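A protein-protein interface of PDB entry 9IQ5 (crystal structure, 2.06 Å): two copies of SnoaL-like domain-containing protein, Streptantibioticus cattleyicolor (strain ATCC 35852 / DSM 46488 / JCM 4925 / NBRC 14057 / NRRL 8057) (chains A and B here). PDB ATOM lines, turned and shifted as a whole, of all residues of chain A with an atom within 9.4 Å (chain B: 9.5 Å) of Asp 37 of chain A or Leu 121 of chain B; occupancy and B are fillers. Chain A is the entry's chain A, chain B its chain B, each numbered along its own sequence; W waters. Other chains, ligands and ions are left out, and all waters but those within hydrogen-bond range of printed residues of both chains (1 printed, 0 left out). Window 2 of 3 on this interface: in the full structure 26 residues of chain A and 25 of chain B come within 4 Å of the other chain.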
ATOM      1  N   THR A  33     -28.774  -0.221  19.837  1.00  0.00           N
ATOM      2  CA  THR A  33     -27.348   0.061  19.686  1.00  0.00           C
ATOM      3  C   THR A  33     -26.769   0.556  21.013  1.00  0.00           C
ATOM      4  O   THR A  33     -27.516   0.900  21.932  1.00  0.00           O
ATOM      5  CB  THR A  33     -27.142   1.132  18.610  1.00  0.00           C
ATOM      6  OG1 THR A  33     -27.598   2.361  19.151  1.00  0.00           O
ATOM      7  CG2 THR A  33     -27.948   0.861  17.342  1.00  0.00           C
ATOM      8  N   PRO A  34     -25.434   0.634  21.131  1.00  0.00           N
ATOM      9  CA  PRO A  34     -24.828   1.037  22.410  1.00  0.00           C
ATOM     10  C   PRO A  34     -24.788   2.531  22.667  1.00  0.00           C
ATOM     11  O   PRO A  34     -24.443   2.931  23.794  1.00  0.00           O
ATOM     12  CB  PRO A  34     -23.395   0.491  22.299  1.00  0.00           C
ATOM     13  CG  PRO A  34     -23.113   0.485  20.842  1.00  0.00           C
ATOM     14  CD  PRO A  34     -24.421   0.143  20.182  1.00  0.00           C
ATOM     15  N   ASP A  35     -25.125   3.363  21.675  1.00  0.00           N
ATOM     16  CA  ASP A  35     -24.870   4.803  21.735  1.00  0.00           C
ATOM     17  C   ASP A  35     -26.218   5.485  21.831  1.00  0.00           C
ATOM     18  O   ASP A  35     -26.841   5.478  22.917  1.00  0.00           O
ATOM     19  CB  ASP A  35     -23.994   5.220  20.544  1.00  0.00           C
ATOM     20  CG  ASP A  35     -22.725   4.353  20.434  1.00  0.00           C
ATOM     21  OD1 ASP A  35     -22.006   4.224  21.459  1.00  0.00           O
ATOM     22  OD2 ASP A  35     -22.469   3.728  19.364  1.00  0.00           O
ATOM     23  N   GLY A  36     -26.738   6.074  20.751  1.00  0.00           N
ATOM     24  CA  GLY A  36     -28.067   6.677  20.789  1.00  0.00           C
ATOM     25  C   GLY A  36     -28.177   7.798  21.795  1.00  0.00           C
ATOM     26  O   GLY A  36     -29.238   7.984  22.415  1.00  0.00           O
ATOM     27  N   ASP A  37     -27.091   8.549  21.975  1.00  0.00           N
ATOM     28  CA  ASP A  37     -27.057   9.720  22.840  1.00  0.00           C
ATOM     29  C   ASP A  37     -27.489   9.392  24.266  1.00  0.00           C
ATOM     30  O   ASP A  37     -28.318  10.084  24.851  1.00  0.00           O
ATOM     31  CB  ASP A  37     -27.906  10.849  22.276  1.00  0.00           C
ATOM     32  CG  ASP A  37     -27.366  12.173  22.666  1.00  0.00           C
ATOM     33  OD1 ASP A  37     -26.135  12.334  22.506  1.00  0.00           O
ATOM     34  OD2 ASP A  37     -28.146  13.034  23.146  1.00  0.00           O
ATOM     35  N   GLY A  38     -26.906   8.333  24.831  1.00  0.00           N
ATOM     36  CA  GLY A  38     -27.196   7.955  26.201  1.00  0.00           C
ATOM     37  C   GLY A  38     -28.482   7.186  26.404  1.00  0.00           C
ATOM     38  O   GLY A  38     -28.751   6.745  27.530  1.00  0.00           O
ATOM     39  N   LEU A  39     -29.287   6.999  25.360  1.00  0.00           N
ATOM     40  CA  LEU A  39     -30.519   6.234  25.467  1.00  0.00           C
ATOM     41  C   LEU A  39     -30.503   4.925  24.679  1.00  0.00           C
ATOM     42  O   LEU A  39     -31.272   4.016  25.012  1.00  0.00           O
ATOM     43  CB  LEU A  39     -31.696   7.089  24.980  1.00  0.00           C
ATOM     44  CG  LEU A  39     -31.959   8.368  25.771  1.00  0.00           C
ATOM     45  CD1 LEU A  39     -33.113   9.118  25.138  1.00  0.00           C
ATOM     46  CD2 LEU A  39     -32.248   8.059  27.251  1.00  0.00           C
ATOM     47  N   GLY A  40     -29.649   4.803  23.659  1.00  0.00           N
ATOM     48  CA  GLY A  40     -29.681   3.659  22.753  1.00  0.00           C
ATOM     49  C   GLY A  40     -30.678   3.867  21.623  1.00  0.00           C
ATOM     50  O   GLY A  40     -31.819   4.255  21.891  1.00  0.00           O
ATOM     51  N   THR A  41     -30.303   3.600  20.364  1.00  0.00           N
ATOM     52  CA  THR A  41     -31.237   3.741  19.244  1.00  0.00           C
ATOM     53  C   THR A  41     -31.974   2.421  19.004  1.00  0.00           C
ATOM     54  O   THR A  41     -31.340   1.386  18.772  1.00  0.00           O
ATOM     55  CB  THR A  41     -30.533   4.128  17.953  1.00  0.00           C
ATOM     56  OG1 THR A  41     -29.711   5.289  18.146  1.00  0.00           O
ATOM     57  CG2 THR A  41     -31.575   4.372  16.858  1.00  0.00           C
ATOM     58  N   VAL A  42     -33.302   2.467  19.015  1.00  0.00           N
ATOM     59  CA  VAL A  42     -34.105   1.272  18.794  1.00  0.00           C
ATOM     60  C   VAL A  42     -34.267   1.054  17.298  1.00  0.00           C
ATOM     61  O   VAL A  42     -34.587   1.989  16.554  1.00  0.00           O
ATOM     62  CB  VAL A  42     -35.470   1.403  19.486  1.00  0.00           C
ATOM     63  CG1 VAL A  42     -36.325   0.154  19.235  1.00  0.00           C
ATOM     64  CG2 VAL A  42     -35.284   1.646  20.981  1.00  0.00           C
ATOM     65  N   VAL A 119     -17.095   2.522  28.221  1.00  0.00           N
ATOM     66  CA  VAL A 119     -17.004   3.875  27.667  1.00  0.00           C
ATOM     67  C   VAL A 119     -15.549   4.331  27.601  1.00  0.00           C
ATOM     68  O   VAL A 119     -14.813   4.248  28.594  1.00  0.00           O
ATOM     69  CB  VAL A 119     -17.838   4.868  28.490  1.00  0.00           C
ATOM     70  CG1 VAL A 119     -17.535   6.281  28.037  1.00  0.00           C
ATOM     71  CG2 VAL A 119     -19.332   4.568  28.346  1.00  0.00           C
ATOM     72  N   LYS A 120     -15.171   4.902  26.450  1.00  0.00           N
ATOM     73  CA  LYS A 120     -13.872   5.492  26.131  1.00  0.00           C
ATOM     74  C   LYS A 120     -13.828   6.994  26.430  1.00  0.00           C
ATOM     75  O   LYS A 120     -14.831   7.624  26.779  1.00  0.00           O
ATOM     76  CB  LYS A 120     -13.519   5.261  24.658  1.00  0.00           C
ATOM     77  CG  LYS A 120     -12.469   4.182  24.400  1.00  0.00           C
ATOM     78  CD  LYS A 120     -11.092   4.646  24.870  1.00  0.00           C
ATOM     79  CE  LYS A 120     -10.674   5.933  24.171  1.00  0.00           C
ATOM     80  NZ  LYS A 120      -9.406   6.526  24.707  1.00  0.00           N
ATOM     81  N   LEU A 121     -12.628   7.565  26.274  1.00  0.00           N
ATOM     82  CA  LEU A 121     -12.322   8.966  26.599  1.00  0.00           C
ATOM     83  C   LEU A 121     -13.381   9.946  26.106  1.00  0.00           C
ATOM     84  O   LEU A 121     -14.014  10.636  26.908  1.00  0.00           O
ATOM     85  CB  LEU A 121     -10.955   9.368  26.002  1.00  0.00           C
ATOM     86  CG  LEU A 121     -10.436  10.796  26.278  1.00  0.00           C
ATOM     87  CD1 LEU A 121      -8.979  10.805  26.742  1.00  0.00           C
ATOM     88  CD2 LEU A 121     -10.594  11.732  25.078  1.00  0.00           C
ATOM     89  N   LYS B  94     -38.300  12.492  32.753  1.00  0.00           N
ATOM     90  CA  LYS B  94     -37.508  12.402  31.544  1.00  0.00           C
ATOM     91  C   LYS B  94     -36.230  11.621  31.804  1.00  0.00           C
ATOM     92  O   LYS B  94     -35.403  12.030  32.623  1.00  0.00           O
ATOM     93  CB  LYS B  94     -37.179  13.794  31.051  1.00  0.00           C
ATOM     94  CG  LYS B  94     -36.239  13.807  29.913  1.00  0.00           C
ATOM     95  CD  LYS B  94     -36.025  15.236  29.501  1.00  0.00           C
ATOM     96  CE  LYS B  94     -34.836  15.362  28.576  1.00  0.00           C
ATOM     97  NZ  LYS B  94     -34.613  16.796  28.328  1.00  0.00           N
ATOM     98  N   VAL B  95     -36.070  10.504  31.109  1.00  0.00           N
ATOM     99  CA  VAL B  95     -34.851   9.709  31.195  1.00  0.00           C
ATOM    100  C   VAL B  95     -33.763  10.375  30.361  1.00  0.00           C
ATOM    101  O   VAL B  95     -33.980  10.708  29.191  1.00  0.00           O
ATOM    102  CB  VAL B  95     -35.124   8.275  30.732  1.00  0.00           C
ATOM    103  CG1 VAL B  95     -33.836   7.464  30.660  1.00  0.00           C
ATOM    104  CG2 VAL B  95     -36.118   7.622  31.680  1.00  0.00           C
ATOM    105  N   VAL B  96     -32.610  10.635  30.983  1.00  0.00           N
ATOM    106  CA  VAL B  96     -31.460  11.188  30.277  1.00  0.00           C
ATOM    107  C   VAL B  96     -30.342  10.178  30.070  1.00  0.00           C
ATOM    108  O   VAL B  96     -29.400  10.479  29.326  1.00  0.00           O
ATOM    109  CB  VAL B  96     -30.898  12.445  30.975  1.00  0.00           C
ATOM    110  CG1 VAL B  96     -31.911  13.572  30.961  1.00  0.00           C
ATOM    111  CG2 VAL B  96     -30.457  12.123  32.378  1.00  0.00           C
ATOM    112  N   ASN B  97     -30.388   9.018  30.717  1.00  0.00           N
ATOM    113  CA  ASN B  97     -29.397   7.969  30.503  1.00  0.00           C
ATOM    114  C   ASN B  97     -29.989   6.657  31.004  1.00  0.00           C
ATOM    115  O   ASN B  97     -30.795   6.658  31.939  1.00  0.00           O
ATOM    116  CB  ASN B  97     -28.067   8.290  31.199  1.00  0.00           C
ATOM    117  CG  ASN B  97     -26.943   7.326  30.826  1.00  0.00           C
ATOM    118  OD1 ASN B  97     -26.147   6.936  31.684  1.00  0.00           O
ATOM    119  ND2 ASN B  97     -26.876   6.929  29.560  1.00  0.00           N
ATOM    120  N   ARG B  98     -29.587   5.544  30.349  1.00  0.00           N
ATOM    121  CA  ARG B  98     -30.039   4.175  30.629  1.00  0.00           C
ATOM    122  C   ARG B  98     -28.851   3.227  30.685  1.00  0.00           C
ATOM    123  O   ARG B  98     -27.849   3.425  29.993  1.00  0.00           O
ATOM    124  CB  ARG B  98     -30.950   3.582  29.528  1.00  0.00           C
ATOM    125  CG  ARG B  98     -32.278   4.243  29.339  1.00  0.00           C
ATOM    126  CD  ARG B  98     -33.114   3.509  28.273  1.00  0.00           C
ATOM    127  NE  ARG B  98     -34.277   4.317  27.908  1.00  0.00           N
ATOM    128  CZ  ARG B  98     -35.367   4.477  28.651  1.00  0.00           C
ATOM    129  NH1 ARG B  98     -35.521   3.853  29.812  1.00  0.00           N
ATOM    130  NH2 ARG B  98     -36.338   5.275  28.210  1.00  0.00           N
ATOM    131  N   ARG B 117     -23.563   1.380  30.560  1.00  0.00           N
ATOM    132  CA  ARG B 117     -24.467   2.480  30.250  1.00  0.00           C
ATOM    133  C   ARG B 117     -24.486   2.714  28.746  1.00  0.00           C
ATOM    134  O   ARG B 117     -23.484   2.471  28.064  1.00  0.00           O
ATOM    135  CB  ARG B 117     -24.046   3.763  30.933  1.00  0.00           C
ATOM    136  CG  ARG B 117     -22.750   4.280  30.399  1.00  0.00           C
ATOM    137  CD  ARG B 117     -22.566   5.761  30.690  1.00  0.00           C
ATOM    138  NE  ARG B 117     -22.015   6.014  32.013  1.00  0.00           N
ATOM    139  CZ  ARG B 117     -22.675   6.586  33.016  1.00  0.00           C
ATOM    140  NH1 ARG B 117     -23.947   6.948  32.900  1.00  0.00           N
ATOM    141  NH2 ARG B 117     -22.040   6.815  34.162  1.00  0.00           N
ATOM    142  N   LYS B 118     -25.642   3.125  28.232  1.00  0.00           N
ATOM    143  CA  LYS B 118     -25.707   3.663  26.884  1.00  0.00           C
ATOM    144  C   LYS B 118     -24.849   4.937  26.795  1.00  0.00           C
ATOM    145  O   LYS B 118     -24.703   5.676  27.764  1.00  0.00           O
ATOM    146  CB  LYS B 118     -27.166   3.926  26.511  1.00  0.00           C
ATOM    147  CG  LYS B 118     -28.066   2.652  26.517  1.00  0.00           C
ATOM    148  CD  LYS B 118     -27.623   1.599  25.475  1.00  0.00           C
ATOM    149  CE  LYS B 118     -28.659   0.457  25.265  1.00  0.00           C
ATOM    150  NZ  LYS B 118     -28.163  -0.543  24.245  1.00  0.00           N
ATOM    151  N   VAL B 119     -24.250   5.174  25.625  1.00  0.00           N
ATOM    152  CA  VAL B 119     -23.192   6.172  25.443  1.00  0.00           C
ATOM    153  C   VAL B 119     -23.724   7.455  24.809  1.00  0.00           C
ATOM    154  O   VAL B 119     -24.579   7.411  23.908  1.00  0.00           O
ATOM    155  CB  VAL B 119     -22.045   5.578  24.600  1.00  0.00           C
ATOM    156  CG1 VAL B 119     -21.019   6.651  24.235  1.00  0.00           C
ATOM    157  CG2 VAL B 119     -21.392   4.401  25.355  1.00  0.00           C
ATOM    158  N   LYS B 120     -23.215   8.608  25.279  1.00  0.00           N
ATOM    159  CA  LYS B 120     -23.446   9.932  24.688  1.00  0.00           C
ATOM    160  C   LYS B 120     -22.349  10.290  23.677  1.00  0.00           C
ATOM    161  O   LYS B 120     -21.284   9.676  23.635  1.00  0.00           O
ATOM    162  CB  LYS B 120     -23.456  11.019  25.765  1.00  0.00           C
ATOM    163  CG  LYS B 120     -24.446  10.782  26.860  1.00  0.00           C
ATOM    164  CD  LYS B 120     -25.149  12.053  27.280  1.00  0.00           C
ATOM    165  CE  LYS B 120     -26.591  11.724  27.569  1.00  0.00           C
ATOM    166  NZ  LYS B 120     -26.641  10.444  28.345  1.00  0.00           N
ATOM    167  N   LEU B 121     -22.602  11.329  22.875  1.00  0.00           N
ATOM    168  CA  LEU B 121     -21.642  11.752  21.829  1.00  0.00           C
ATOM    169  C   LEU B 121     -20.234  11.956  22.387  1.00  0.00           C
ATOM    170  O   LEU B 121     -20.004  12.894  23.144  1.00  0.00           O
ATOM    171  CB  LEU B 121     -22.107  13.029  21.133  1.00  0.00           C
ATOM    172  CG  LEU B 121     -21.244  13.562  19.971  1.00  0.00           C
ATOM    173  CD1 LEU B 121     -20.148  14.593  20.399  1.00  0.00           C
ATOM    174  CD2 LEU B 121     -20.642  12.402  19.148  1.00  0.00           C
HETATM  175  O   HOH W   1     -23.362   1.236  25.528  1.00  0.00           O
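The backbone carbonyl oxygen (O) of Thr 33 of chain A sits at hydrogen-bond distance from the side-chain amino group (NZ) of Lys 118 of chain B, at 2.8 Å. The backbone carbonyl oxygen of Pro 34 of chain A is in hydrogen-bond range of the backbone NH of Val 119 of chain B (2.9 Å). O of Val 119 of chain B lies within hydrogen-bond range of N of Asp 37 of chain A, at 3.4 Å. The backbone carbonyl oxygen (O) of Gly 38 of chain A lies within hydrogen-bond range of the side-chain amide nitrogen (ND2) of Asn 97 of chain B. The backbone carbonyl oxygen (O) of Gly 38 of chain A sits at hydrogen-bond distance from the backbone NH (N) of Arg 98 of chain B (3.2 Å). The backbone NH (N) of Gly 38 of chain A sits at hydrogen-bond distance from the backbone carbonyl oxygen (O) of Val 119 of chain B (2.7 Å). The backbone carbonyl oxygen (O) of Asp 35 of chain A sits close to the backbone carbonyl oxygen (O) of Val 119 of chain B, 3.1 Å away.
Val 119 of chain B touches its own counterpart, Val 119 of chain A. Positions printed for both chains: 119, 120 and 121.
Of the printed residues of chain B, Thr 33 of chain A touches Lys 118 (2.8 Å). Printed residues of chain B within 4 Å of Asp 37 of chain A: Val 119, Lys 120 and Leu 121. Of chain B, only Asn 97 (2.8 Å), Arg 98 (3.2 Å), Lys 118 (3.4 Å), Val 119 (2.7 Å) and Lys 120 (3.3 Å) come within 4 Å of Gly 38 of chain A. Of the printed residues of chain B, Val 119 of chain A touches Arg 117 and Val 119. Printed residues of chain A within 4 Å of Val 119 of chain B: Pro 34 (2.9 Å), Asp 35 (3.1 Å), Asp 37 (3.4 Å), Gly 38 (2.7 Å) and Val 119 (3.6 Å). Of chain A, only Asp 37 comes within 4 Å of Leu 121 of chain B. The nearest residue of chain B that does not touch Asp 37 of chain A is Val 96 of chain B (4.6 Å). The nearest printed residue of chain B that does not touch Gly 40 of chain A is Val 119 of chain B (5.7 Å).
Printed residues of chain A that touch a printed residue of chain B: Thr 33, Pro 34, Asp 35, Asp 37, Gly 38, Leu 39, Gly 40 and Val 119. Hydrophobic or aromatic side chains of chain A that line the printed part of chain B: Leu 39 and Val 119. Along chain A the printed residues that touch a printed residue of chain B span positions 33 to 119. Printed residues of chain B that touch a printed residue of chain A: Val 95, Asn 97, Arg 98, Arg 117, Lys 118, Val 119, Lys 120 and Leu 121. Hydrophobic or aromatic side chains of chain B that line the printed part of chain A: Val 95 and Val 119. Among the printed residues, no Asp or Glu carboxylate lies within 4 Å of a Lys or Arg side-chain nitrogen of the other chain.
The backbone NH (N) of Thr 33 of chain A is in hydrogen-bond range of the backbone carbonyl oxygen (O) of Thr 41 of chain A (3.2 Å). O of Asp 35 of chain A sits at hydrogen-bond distance from N of Gly 40 of chain A (3.0 Å). O of Val 96 of chain B is in hydrogen-bond range of NZ of Lys 120 of chain B, 2.9 Å away. The guanidinium group (NH1) of Arg 117 of chain B sits at hydrogen-bond distance from the side-chain amide oxygen (OD1) of Asn 97 of chain B (2.5 Å). The backbone carbonyl oxygen (O) of Lys 118 of chain B lies within hydrogen-bond range of the side-chain amide nitrogen (ND2) of Asn 97 of chain B (3.1 Å). The backbone NH (N) of Lys 118 of chain B lies within hydrogen-bond range of the backbone carbonyl oxygen (O) of Arg 98 of chain B, 2.8 Å away.
Lys 118 of chain B touches Pro 34 of chain A (CA to O, 3.4 Å). Lys 118 of chain B touches Asp 35 of chain A. Asp 37 of chain A touches Lys 120 of chain B (O to CE, 3.6 Å). Lys 118 of chain B touches Gly 38 of chain A. Gly 38 of chain A touches Lys 120 of chain B. Leu 39 of chain A touches Val 95 of chain B. Leu 39 of chain A touches Lys 118 of chain B. Gly 40 of chain A touches Lys 118 of chain B (N to CB, 3.9 Å). CG2 of Val 119 of chain A touches CG of Arg 117 of chain B (3.998 Å). Val 119 of chain A touches Val 119 of chain B (CG2 to CG2, 3.6 Å).
Water W1 bridges the backbone carbonyl oxygen (O) of Pro 34 of chain A (2.7 Å) and the backbone carbonyl oxygen (O) of Arg 117 of chain B (2.8 Å).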
